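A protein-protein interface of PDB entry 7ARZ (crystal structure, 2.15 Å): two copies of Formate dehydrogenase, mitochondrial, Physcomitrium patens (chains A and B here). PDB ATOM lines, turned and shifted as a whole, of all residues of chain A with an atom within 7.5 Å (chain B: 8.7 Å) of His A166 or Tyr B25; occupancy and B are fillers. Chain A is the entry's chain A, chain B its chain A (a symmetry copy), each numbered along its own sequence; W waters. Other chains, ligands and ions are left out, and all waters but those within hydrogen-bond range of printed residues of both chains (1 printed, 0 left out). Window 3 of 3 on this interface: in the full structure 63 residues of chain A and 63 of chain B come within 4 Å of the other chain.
N of Leu B321 sits at hydrogen-bond distance from O of Ala A168, at 3.0 Å.
The side-chain amide oxygen (OE1) of Gln B324 lies within hydrogen-bond range of the backbone NH (N) of Leu B32.
SG of Cys B34 lies within hydrogen-bond range of O of Phe B31.
O of Thr B319 sits at hydrogen-bond distance from NE2 of Gln B324, at 3.0 Å.
The side-chain amide oxygen of Asn A160 is in hydrogen-bond range of the backbone NH of Ala A163 (3.2 Å).
N of Ala A162 sits close to OD1 of Asn A160 (3.3 Å).
ND2 of Asn A146 is in hydrogen-bond range of O of Val A164.
Among the printed residues, merely in contact across the chains: Val A161 with Phe B20, Val A161 with Thr B319, Ala A162 with Ala B21, Ala A162 with Ala B22, Ala A162 with Tyr B25, Ala A162 with Phe B31, Ala A163 with Tyr B25, Val A164 with Ile B316, Val A165 with Phe B31, Val A165 with Ile B316, Val A165 with Thr B319, Val A165 with Leu B321, Val A165 with Gln B324, His A166 with Tyr B25, His A166 with Phe B31, His A166 with Leu B321, Ala A168 with Thr B320, Tyr A169 with Thr B320 and Tyr A169 with Leu B321.
His A166 touches just these residues of chain B: Tyr B25 (3.2 Å), Phe B31 (3.9 Å) and Leu B321 (3.6 Å).
Tyr B25 touches just these residues of chain A: Ala A162 (3.96 Å), Ala A163 (3.7 Å) and His A166 (3.2 Å).
Of the printed residues of chain B, Ala A163 touches Tyr B25 (3.7 Å).
Printed residues of chain B within 4 Å of Val A161: Phe B20 and Thr B319.
Printed residues of chain A within 4 Å of Phe B20: Val A161 (3.6 Å).
His A167 touches none of the printed residues of chain B.
Glu B30 touches none of the printed residues of chain A.
The nearest residue of chain A that does not touch Tyr B25 is Asn A160 (5.3 Å).
The nearest printed residue of chain B that does not touch Ala A168 is Thr B319 (5.4 Å).
Hydrophobic or aromatic side chains of chain B that line the printed part of chain A: Phe B20, Tyr B25, Phe B31, Ile B316 and Leu B321.
Of the 12 printed residues of chain A, 8 touch a printed residue of chain B.
Among the printed residues, 20 pairs touch across the chains.
Among the printed residues, no Asp or Glu carboxylate lies within 4 Å of a Lys or Arg side-chain nitrogen of the other chain.
No position is printed for both chains.
Water W1 lies within hydrogen-bond range of the backbone NH of Ala A162, the side-chain amide oxygen of Asn A160, the backbone carbonyl oxygen of Ala B21 and the backbone NH of Val A161.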
ATOM      1  N   ASN A 146     -14.784 -24.004  -7.032  1.00  0.00           N
ATOM      2  CA  ASN A 146     -14.545 -23.223  -5.797  1.00  0.00           C
ATOM      3  C   ASN A 146     -14.163 -21.768  -6.076  1.00  0.00           C
ATOM      4  O   ASN A 146     -13.293 -21.225  -5.353  1.00  0.00           O
ATOM      5  CB  ASN A 146     -13.467 -23.883  -4.944  1.00  0.00           C
ATOM      6  CG  ASN A 146     -13.681 -23.601  -3.474  1.00  0.00           C
ATOM      7  OD1 ASN A 146     -14.794 -23.329  -3.049  1.00  0.00           O
ATOM      8  ND2 ASN A 146     -12.619 -23.626  -2.702  1.00  0.00           N
ATOM      9  N   ASN A 160      -3.364 -17.468  -1.316  1.00  0.00           N
ATOM     10  CA  ASN A 160      -3.226 -18.865  -0.864  1.00  0.00           C
ATOM     11  C   ASN A 160      -3.973 -19.737  -1.868  1.00  0.00           C
ATOM     12  O   ASN A 160      -5.196 -19.910  -1.741  1.00  0.00           O
ATOM     13  CB  ASN A 160      -3.678 -19.002   0.589  1.00  0.00           C
ATOM     14  CG  ASN A 160      -3.315 -20.348   1.165  1.00  0.00           C
ATOM     15  OD1 ASN A 160      -2.950 -21.252   0.421  1.00  0.00           O
ATOM     16  ND2 ASN A 160      -3.429 -20.487   2.472  1.00  0.00           N
ATOM     17  N   VAL A 161      -3.256 -20.273  -2.840  1.00  0.00           N
ATOM     18  CA  VAL A 161      -3.870 -21.130  -3.886  1.00  0.00           C
ATOM     19  C   VAL A 161      -4.450 -22.386  -3.228  1.00  0.00           C
ATOM     20  O   VAL A 161      -5.596 -22.786  -3.577  1.00  0.00           O
ATOM     21  CB  VAL A 161      -2.836 -21.431  -4.973  1.00  0.00           C
ATOM     22  CG1 VAL A 161      -3.375 -22.399  -6.015  1.00  0.00           C
ATOM     23  CG2 VAL A 161      -2.355 -20.144  -5.618  1.00  0.00           C
ATOM     24  N   ALA A 162      -3.744 -22.944  -2.244  1.00  0.00           N
ATOM     25  CA  ALA A 162      -4.111 -24.218  -1.598  1.00  0.00           C
ATOM     26  C   ALA A 162      -5.450 -24.074  -0.882  1.00  0.00           C
ATOM     27  O   ALA A 162      -6.262 -25.025  -0.957  1.00  0.00           O
ATOM     28  CB  ALA A 162      -3.035 -24.643  -0.624  1.00  0.00           C
ATOM     29  N   ALA A 163      -5.642 -22.981  -0.136  1.00  0.00           N
ATOM     30  CA  ALA A 163      -6.863 -22.785   0.678  1.00  0.00           C
ATOM     31  C   ALA A 163      -8.104 -22.800  -0.227  1.00  0.00           C
ATOM     32  O   ALA A 163      -9.195 -22.930   0.343  1.00  0.00           O
ATOM     33  CB  ALA A 163      -6.790 -21.515   1.491  1.00  0.00           C
ATOM     34  N   VAL A 164      -7.939 -22.682  -1.558  1.00  0.00           N
ATOM     35  CA  VAL A 164      -9.020 -22.731  -2.581  1.00  0.00           C
ATOM     36  C   VAL A 164      -9.012 -24.117  -3.231  1.00  0.00           C
ATOM     37  O   VAL A 164     -10.056 -24.787  -3.178  1.00  0.00           O
ATOM     38  CB  VAL A 164      -8.865 -21.621  -3.649  1.00  0.00           C
ATOM     39  CG1 VAL A 164      -9.902 -21.722  -4.761  1.00  0.00           C
ATOM     40  CG2 VAL A 164      -8.920 -20.234  -3.025  1.00  0.00           C
ATOM     41  N   VAL A 165      -7.902 -24.521  -3.858  1.00  0.00           N
ATOM     42  CA  VAL A 165      -7.891 -25.730  -4.735  1.00  0.00           C
ATOM     43  C   VAL A 165      -7.901 -27.022  -3.902  1.00  0.00           C
ATOM     44  O   VAL A 165      -8.055 -28.087  -4.480  1.00  0.00           O
ATOM     45  CB  VAL A 165      -6.751 -25.692  -5.769  1.00  0.00           C
ATOM     46  CG1 VAL A 165      -6.876 -24.451  -6.660  1.00  0.00           C
ATOM     47  CG2 VAL A 165      -5.372 -25.798  -5.130  1.00  0.00           C
ATOM     48  N   HIS A 166      -7.846 -26.958  -2.581  1.00  0.00           N
ATOM     49  CA  HIS A 166      -8.024 -28.184  -1.767  1.00  0.00           C
ATOM     50  C   HIS A 166      -9.455 -28.662  -1.925  1.00  0.00           C
ATOM     51  O   HIS A 166      -9.729 -29.802  -1.526  1.00  0.00           O
ATOM     52  CB  HIS A 166      -7.695 -27.958  -0.294  1.00  0.00           C
ATOM     53  CG  HIS A 166      -8.794 -27.358   0.492  1.00  0.00           C
ATOM     54  ND1 HIS A 166      -9.694 -28.128   1.197  1.00  0.00           N
ATOM     55  CD2 HIS A 166      -9.121 -26.070   0.724  1.00  0.00           C
ATOM     56  CE1 HIS A 166     -10.553 -27.341   1.815  1.00  0.00           C
ATOM     57  NE2 HIS A 166     -10.224 -26.072   1.541  1.00  0.00           N
ATOM     58  N   HIS A 167     -10.340 -27.804  -2.448  1.00  0.00           N
ATOM     59  CA  HIS A 167     -11.784 -28.128  -2.637  1.00  0.00           C
ATOM     60  C   HIS A 167     -12.228 -27.649  -4.010  1.00  0.00           C
ATOM     61  O   HIS A 167     -13.348 -27.171  -4.115  1.00  0.00           O
ATOM     62  CB  HIS A 167     -12.649 -27.530  -1.508  1.00  0.00           C
ATOM     63  CG  HIS A 167     -14.048 -28.050  -1.466  1.00  0.00           C
ATOM     64  ND1 HIS A 167     -14.342 -29.393  -1.487  1.00  0.00           N
ATOM     65  CD2 HIS A 167     -15.231 -27.412  -1.352  1.00  0.00           C
ATOM     66  CE1 HIS A 167     -15.651 -29.565  -1.419  1.00  0.00           C
ATOM     67  NE2 HIS A 167     -16.217 -28.359  -1.314  1.00  0.00           N
ATOM     68  N   ALA A 168     -11.373 -27.777  -5.013  1.00  0.00           N
ATOM     69  CA  ALA A 168     -11.692 -27.349  -6.393  1.00  0.00           C
ATOM     70  C   ALA A 168     -11.437 -28.502  -7.336  1.00  0.00           C
ATOM     71  O   ALA A 168     -10.339 -29.084  -7.265  1.00  0.00           O
ATOM     72  CB  ALA A 168     -10.887 -26.141  -6.813  1.00  0.00           C
ATOM     73  N   TYR A 169     -12.406 -28.758  -8.204  1.00  0.00           N
ATOM     74  CA  TYR A 169     -12.445 -29.901  -9.142  1.00  0.00           C
ATOM     75  C   TYR A 169     -12.838 -29.377 -10.518  1.00  0.00           C
ATOM     76  O   TYR A 169     -13.172 -28.192 -10.648  1.00  0.00           O
ATOM     77  CB  TYR A 169     -13.395 -30.974  -8.601  1.00  0.00           C
ATOM     78  CG  TYR A 169     -13.120 -31.368  -7.168  1.00  0.00           C
ATOM     79  CD1 TYR A 169     -13.636 -30.627  -6.123  1.00  0.00           C
ATOM     80  CD2 TYR A 169     -12.315 -32.456  -6.847  1.00  0.00           C
ATOM     81  CE1 TYR A 169     -13.388 -30.973  -4.803  1.00  0.00           C
ATOM     82  CE2 TYR A 169     -12.058 -32.818  -5.527  1.00  0.00           C
ATOM     83  CZ  TYR A 169     -12.589 -32.067  -4.497  1.00  0.00           C
ATOM     84  OH  TYR A 169     -12.351 -32.362  -3.181  1.00  0.00           O
ATOM     85  N   ASN A 309     -19.272 -23.375   1.949  1.00  0.00           N
ATOM     86  CA  ASN A 309     -19.288 -23.786   0.517  1.00  0.00           C
ATOM     87  C   ASN A 309     -20.623 -23.402  -0.162  1.00  0.00           C
ATOM     88  O   ASN A 309     -21.172 -24.222  -0.948  1.00  0.00           O
ATOM     89  CB  ASN A 309     -18.934 -25.264   0.420  1.00  0.00           C
ATOM     90  CG  ASN A 309     -17.513 -25.520   0.876  1.00  0.00           C
ATOM     91  OD1 ASN A 309     -16.669 -24.642   0.777  1.00  0.00           O
ATOM     92  ND2 ASN A 309     -17.235 -26.720   1.360  1.00  0.00           N
ATOM     93  N   PHE B  20       3.990 -24.241  -4.499  1.00  0.00           N
ATOM     94  CA  PHE B  20       3.405 -23.550  -3.319  1.00  0.00           C
ATOM     95  C   PHE B  20       3.256 -24.557  -2.192  1.00  0.00           C
ATOM     96  O   PHE B  20       3.134 -25.765  -2.456  1.00  0.00           O
ATOM     97  CB  PHE B  20       2.076 -22.856  -3.641  1.00  0.00           C
ATOM     98  CG  PHE B  20       0.966 -23.722  -4.193  1.00  0.00           C
ATOM     99  CD1 PHE B  20       0.237 -24.560  -3.369  1.00  0.00           C
ATOM    100  CD2 PHE B  20       0.638 -23.663  -5.529  1.00  0.00           C
ATOM    101  CE1 PHE B  20      -0.787 -25.340  -3.886  1.00  0.00           C
ATOM    102  CE2 PHE B  20      -0.391 -24.429  -6.044  1.00  0.00           C
ATOM    103  CZ  PHE B  20      -1.111 -25.248  -5.221  1.00  0.00           C
ATOM    104  N   ALA B  21       3.218 -24.072  -0.964  1.00  0.00           N
ATOM    105  CA  ALA B  21       2.888 -24.884   0.228  1.00  0.00           C
ATOM    106  C   ALA B  21       1.373 -25.118   0.272  1.00  0.00           C
ATOM    107  O   ALA B  21       0.606 -24.176  -0.061  1.00  0.00           O
ATOM    108  CB  ALA B  21       3.387 -24.185   1.473  1.00  0.00           C
ATOM    109  N   ALA B  22       0.949 -26.333   0.626  1.00  0.00           N
ATOM    110  CA  ALA B  22      -0.465 -26.699   0.868  1.00  0.00           C
ATOM    111  C   ALA B  22      -0.719 -26.849   2.366  1.00  0.00           C
ATOM    112  O   ALA B  22      -1.892 -27.024   2.746  1.00  0.00           O
ATOM    113  CB  ALA B  22      -0.819 -27.954   0.100  1.00  0.00           C
ATOM    114  N   HIS B  23       0.333 -26.768   3.189  1.00  0.00           N
ATOM    115  CA  HIS B  23       0.295 -27.031   4.654  1.00  0.00           C
ATOM    116  C   HIS B  23      -0.676 -28.195   4.915  1.00  0.00           C
ATOM    117  O   HIS B  23      -0.484 -29.249   4.275  1.00  0.00           O
ATOM    118  CB  HIS B  23       0.014 -25.739   5.429  1.00  0.00           C
ATOM    119  CG  HIS B  23       0.924 -24.635   5.028  1.00  0.00           C
ATOM    120  ND1 HIS B  23       2.245 -24.592   5.425  1.00  0.00           N
ATOM    121  CD2 HIS B  23       0.733 -23.568   4.223  1.00  0.00           C
ATOM    122  CE1 HIS B  23       2.833 -23.533   4.908  1.00  0.00           C
ATOM    123  NE2 HIS B  23       1.924 -22.886   4.165  1.00  0.00           N
ATOM    124  N   GLU B  24      -1.680 -28.025   5.780  1.00  0.00           N
ATOM    125  CA  GLU B  24      -2.580 -29.122   6.214  1.00  0.00           C
ATOM    126  C   GLU B  24      -3.310 -29.735   5.012  1.00  0.00           C
ATOM    127  O   GLU B  24      -3.654 -30.926   5.096  1.00  0.00           O
ATOM    128  CB  GLU B  24      -3.524 -28.664   7.335  1.00  0.00           C
ATOM    129  CG  GLU B  24      -4.663 -27.751   6.893  1.00  0.00           C
ATOM    130  CD  GLU B  24      -4.493 -26.250   7.111  1.00  0.00           C
ATOM    131  OE1 GLU B  24      -3.405 -25.703   6.781  1.00  0.00           O
ATOM    132  OE2 GLU B  24      -5.470 -25.622   7.589  1.00  0.00           O
ATOM    133  N   TYR B  25      -3.520 -29.004   3.910  1.00  0.00           N
ATOM    134  CA  TYR B  25      -4.293 -29.525   2.745  1.00  0.00           C
ATOM    135  C   TYR B  25      -3.511 -30.639   2.047  1.00  0.00           C
ATOM    136  O   TYR B  25      -4.128 -31.368   1.237  1.00  0.00           O
ATOM    137  CB  TYR B  25      -4.713 -28.401   1.796  1.00  0.00           C
ATOM    138  CG  TYR B  25      -5.559 -27.369   2.488  1.00  0.00           C
ATOM    139  CD1 TYR B  25      -6.799 -27.708   3.011  1.00  0.00           C
ATOM    140  CD2 TYR B  25      -5.097 -26.075   2.677  1.00  0.00           C
ATOM    141  CE1 TYR B  25      -7.578 -26.772   3.676  1.00  0.00           C
ATOM    142  CE2 TYR B  25      -5.860 -25.133   3.346  1.00  0.00           C
ATOM    143  CZ  TYR B  25      -7.107 -25.481   3.836  1.00  0.00           C
ATOM    144  OH  TYR B  25      -7.845 -24.549   4.503  1.00  0.00           O
ATOM    145  N   ALA B  26      -2.219 -30.784   2.365  1.00  0.00           N
ATOM    146  CA  ALA B  26      -1.328 -31.837   1.812  1.00  0.00           C
ATOM    147  C   ALA B  26      -1.695 -33.223   2.361  1.00  0.00           C
ATOM    148  O   ALA B  26      -1.225 -34.204   1.748  1.00  0.00           O
ATOM    149  CB  ALA B  26       0.124 -31.519   2.078  1.00  0.00           C
ATOM    150  N   LYS B  27      -2.508 -33.289   3.429  1.00  0.00           N
ATOM    151  CA  LYS B  27      -3.071 -34.538   4.006  1.00  0.00           C
ATOM    152  C   LYS B  27      -3.876 -35.289   2.939  1.00  0.00           C
ATOM    153  O   LYS B  27      -4.040 -36.513   3.065  1.00  0.00           O
ATOM    154  CB  LYS B  27      -3.956 -34.227   5.212  1.00  0.00           C
ATOM    155  CG  LYS B  27      -3.238 -33.886   6.512  1.00  0.00           C
ATOM    156  CD  LYS B  27      -4.234 -33.594   7.637  1.00  0.00           C
ATOM    157  CE  LYS B  27      -3.633 -33.580   9.029  1.00  0.00           C
ATOM    158  NZ  LYS B  27      -2.736 -32.415   9.214  1.00  0.00           N
ATOM    159  N   ASN B  28      -4.387 -34.592   1.927  1.00  0.00           N
ATOM    160  CA  ASN B  28      -5.035 -35.261   0.773  1.00  0.00           C
ATOM    161  C   ASN B  28      -3.938 -35.621  -0.225  1.00  0.00           C
ATOM    162  O   ASN B  28      -3.420 -34.744  -0.911  1.00  0.00           O
ATOM    163  CB  ASN B  28      -6.157 -34.411   0.164  1.00  0.00           C
ATOM    164  CG  ASN B  28      -6.737 -35.044  -1.082  1.00  0.00           C
ATOM    165  OD1 ASN B  28      -6.324 -36.127  -1.474  1.00  0.00           O
ATOM    166  ND2 ASN B  28      -7.661 -34.362  -1.738  1.00  0.00           N
ATOM    167  N   PRO B  29      -3.561 -36.911  -0.370  1.00  0.00           N
ATOM    168  CA  PRO B  29      -2.536 -37.298  -1.338  1.00  0.00           C
ATOM    169  C   PRO B  29      -2.912 -37.025  -2.805  1.00  0.00           C
ATOM    170  O   PRO B  29      -1.995 -36.977  -3.611  1.00  0.00           O
ATOM    171  CB  PRO B  29      -2.356 -38.807  -1.108  1.00  0.00           C
ATOM    172  CG  PRO B  29      -3.672 -39.246  -0.487  1.00  0.00           C
ATOM    173  CD  PRO B  29      -4.099 -38.065   0.364  1.00  0.00           C
ATOM    174  N   GLU B  30      -4.197 -36.842  -3.150  1.00  0.00           N
ATOM    175  CA  GLU B  30      -4.553 -36.393  -4.532  1.00  0.00           C
ATOM    176  C   GLU B  30      -3.984 -34.978  -4.719  1.00  0.00           C
ATOM    177  O   GLU B  30      -3.897 -34.536  -5.862  1.00  0.00           O
ATOM    178  CB  GLU B  30      -6.023 -36.121  -4.880  1.00  0.00           C
ATOM    179  CG  GLU B  30      -7.127 -37.136  -4.639  1.00  0.00           C
ATOM    180  CD  GLU B  30      -8.469 -36.401  -4.808  1.00  0.00           C
ATOM    181  OE1 GLU B  30      -8.869 -36.100  -5.965  1.00  0.00           O
ATOM    182  OE2 GLU B  30      -9.051 -36.003  -3.798  1.00  0.00           O
ATOM    183  N   PHE B  31      -3.731 -34.248  -3.629  1.00  0.00           N
ATOM    184  CA  PHE B  31      -3.152 -32.880  -3.688  1.00  0.00           C
ATOM    185  C   PHE B  31      -1.654 -33.021  -3.968  1.00  0.00           C
ATOM    186  O   PHE B  31      -0.816 -32.730  -3.071  1.00  0.00           O
ATOM    187  CB  PHE B  31      -3.438 -32.042  -2.434  1.00  0.00           C
ATOM    188  CG  PHE B  31      -3.358 -30.543  -2.653  1.00  0.00           C
ATOM    189  CD1 PHE B  31      -2.545 -29.995  -3.634  1.00  0.00           C
ATOM    190  CD2 PHE B  31      -4.132 -29.677  -1.891  1.00  0.00           C
ATOM    191  CE1 PHE B  31      -2.513 -28.624  -3.836  1.00  0.00           C
ATOM    192  CE2 PHE B  31      -4.126 -28.305  -2.116  1.00  0.00           C
ATOM    193  CZ  PHE B  31      -3.291 -27.779  -3.067  1.00  0.00           C
ATOM    194  N   LEU B  32      -1.360 -33.422  -5.206  1.00  0.00           N
ATOM    195  CA  LEU B  32      -0.010 -33.694  -5.748  1.00  0.00           C
ATOM    196  C   LEU B  32       0.764 -32.382  -5.940  1.00  0.00           C
ATOM    197  O   LEU B  32       2.000 -32.375  -5.680  1.00  0.00           O
ATOM    198  CB  LEU B  32      -0.173 -34.447  -7.076  1.00  0.00           C
ATOM    199  CG  LEU B  32      -0.746 -35.867  -6.950  1.00  0.00           C
ATOM    200  CD1 LEU B  32      -1.143 -36.428  -8.305  1.00  0.00           C
ATOM    201  CD2 LEU B  32       0.245 -36.802  -6.260  1.00  0.00           C
ATOM    202  N   CYS B  34       1.911 -29.545  -4.824  1.00  0.00           N
ATOM    203  CA  CYS B  34       2.287 -28.753  -3.636  1.00  0.00           C
ATOM    204  C   CYS B  34       3.676 -29.197  -3.180  1.00  0.00           C
ATOM    205  O   CYS B  34       4.133 -30.246  -3.638  1.00  0.00           O
ATOM    206  CB  CYS B  34       1.217 -28.846  -2.565  1.00  0.00           C
ATOM    207  SG  CYS B  34       1.177 -30.389  -1.629  1.00  0.00           S
ATOM    208  N   GLU B  36       4.801 -30.148  -0.337  1.00  0.00           N
ATOM    209  CA  GLU B  36       4.760 -31.273   0.636  1.00  0.00           C
ATOM    210  C   GLU B  36       4.681 -32.617  -0.107  1.00  0.00           C
ATOM    211  O   GLU B  36       5.426 -33.527   0.279  1.00  0.00           O
ATOM    212  CB  GLU B  36       3.610 -31.136   1.629  1.00  0.00           C
ATOM    213  CG  GLU B  36       3.737 -29.942   2.551  1.00  0.00           C
ATOM    214  CD  GLU B  36       3.093 -28.643   2.055  1.00  0.00           C
ATOM    215  OE1 GLU B  36       2.631 -28.581   0.887  1.00  0.00           O
ATOM    216  OE2 GLU B  36       3.076 -27.686   2.831  1.00  0.00           O
ATOM    217  N   ASN B  37       3.851 -32.739  -1.145  1.00  0.00           N
ATOM    218  CA  ASN B  37       3.649 -34.026  -1.869  1.00  0.00           C
ATOM    219  C   ASN B  37       4.463 -34.036  -3.164  1.00  0.00           C
ATOM    220  O   ASN B  37       4.680 -35.126  -3.701  1.00  0.00           O
ATOM    221  CB  ASN B  37       2.172 -34.322  -2.142  1.00  0.00           C
ATOM    222  CG  ASN B  37       1.373 -34.429  -0.866  1.00  0.00           C
ATOM    223  OD1 ASN B  37       1.924 -34.752   0.184  1.00  0.00           O
ATOM    224  ND2 ASN B  37       0.082 -34.137  -0.944  1.00  0.00           N
ATOM    225  N   ILE B 316      -5.838 -20.432  -9.828  1.00  0.00           N
ATOM    226  CA  ILE B 316      -6.506 -21.685  -9.380  1.00  0.00           C
ATOM    227  C   ILE B 316      -6.942 -22.546 -10.573  1.00  0.00           C
ATOM    228  O   ILE B 316      -6.948 -23.787 -10.428  1.00  0.00           O
ATOM    229  CB  ILE B 316      -7.672 -21.338  -8.450  1.00  0.00           C
ATOM    230  CG1 ILE B 316      -8.715 -20.441  -9.120  1.00  0.00           C
ATOM    231  CG2 ILE B 316      -7.124 -20.693  -7.190  1.00  0.00           C
ATOM    232  CD1 ILE B 316      -9.940 -20.269  -8.299  1.00  0.00           C
ATOM    233  N   THR B 319      -5.085 -25.713 -11.777  1.00  0.00           N
ATOM    234  CA  THR B 319      -4.556 -26.473 -10.612  1.00  0.00           C
ATOM    235  C   THR B 319      -5.704 -26.865  -9.677  1.00  0.00           C
ATOM    236  O   THR B 319      -5.497 -26.962  -8.467  1.00  0.00           O
ATOM    237  CB  THR B 319      -3.486 -25.683  -9.848  1.00  0.00           C
ATOM    238  OG1 THR B 319      -3.034 -26.447  -8.730  1.00  0.00           O
ATOM    239  CG2 THR B 319      -3.984 -24.348  -9.331  1.00  0.00           C
ATOM    240  N   THR B 320      -6.873 -27.174 -10.230  1.00  0.00           N
ATOM    241  CA  THR B 320      -7.874 -28.005  -9.528  1.00  0.00           C
ATOM    242  C   THR B 320      -7.225 -29.376  -9.277  1.00  0.00           C
ATOM    243  O   THR B 320      -6.279 -29.728 -10.004  1.00  0.00           O
ATOM    244  CB  THR B 320      -9.150 -28.179 -10.342  1.00  0.00           C
ATOM    245  OG1 THR B 320      -8.750 -28.978 -11.449  1.00  0.00           O
ATOM    246  CG2 THR B 320      -9.775 -26.878 -10.810  1.00  0.00           C
ATOM    247  N   LEU B 321      -7.727 -30.118  -8.295  1.00  0.00           N
ATOM    248  CA  LEU B 321      -7.253 -31.491  -7.971  1.00  0.00           C
ATOM    249  C   LEU B 321      -7.235 -32.343  -9.245  1.00  0.00           C
ATOM    250  O   LEU B 321      -6.261 -33.097  -9.423  1.00  0.00           O
ATOM    251  CB  LEU B 321      -8.143 -32.047  -6.864  1.00  0.00           C
ATOM    252  CG  LEU B 321      -7.892 -31.381  -5.513  1.00  0.00           C
ATOM    253  CD1 LEU B 321      -8.955 -31.761  -4.481  1.00  0.00           C
ATOM    254  CD2 LEU B 321      -6.501 -31.726  -5.005  1.00  0.00           C
ATOM    255  N   GLN B 324      -4.264 -31.270 -11.433  1.00  0.00           N
ATOM    256  CA  GLN B 324      -2.996 -31.660 -10.759  1.00  0.00           C
ATOM    257  C   GLN B 324      -2.604 -33.077 -11.165  1.00  0.00           C
ATOM    258  O   GLN B 324      -1.423 -33.286 -11.512  1.00  0.00           O
ATOM    259  CB  GLN B 324      -3.146 -31.557  -9.245  1.00  0.00           C
ATOM    260  CG  GLN B 324      -3.096 -30.121  -8.758  1.00  0.00           C
ATOM    261  CD  GLN B 324      -3.318 -30.024  -7.276  1.00  0.00           C
ATOM    262  OE1 GLN B 324      -2.682 -30.716  -6.489  1.00  0.00           O
ATOM    263  NE2 GLN B 324      -4.238 -29.172  -6.873  1.00  0.00           N
HETATM  264  O   HOH W   1      -1.020 -22.241  -1.516  1.00  0.00           O
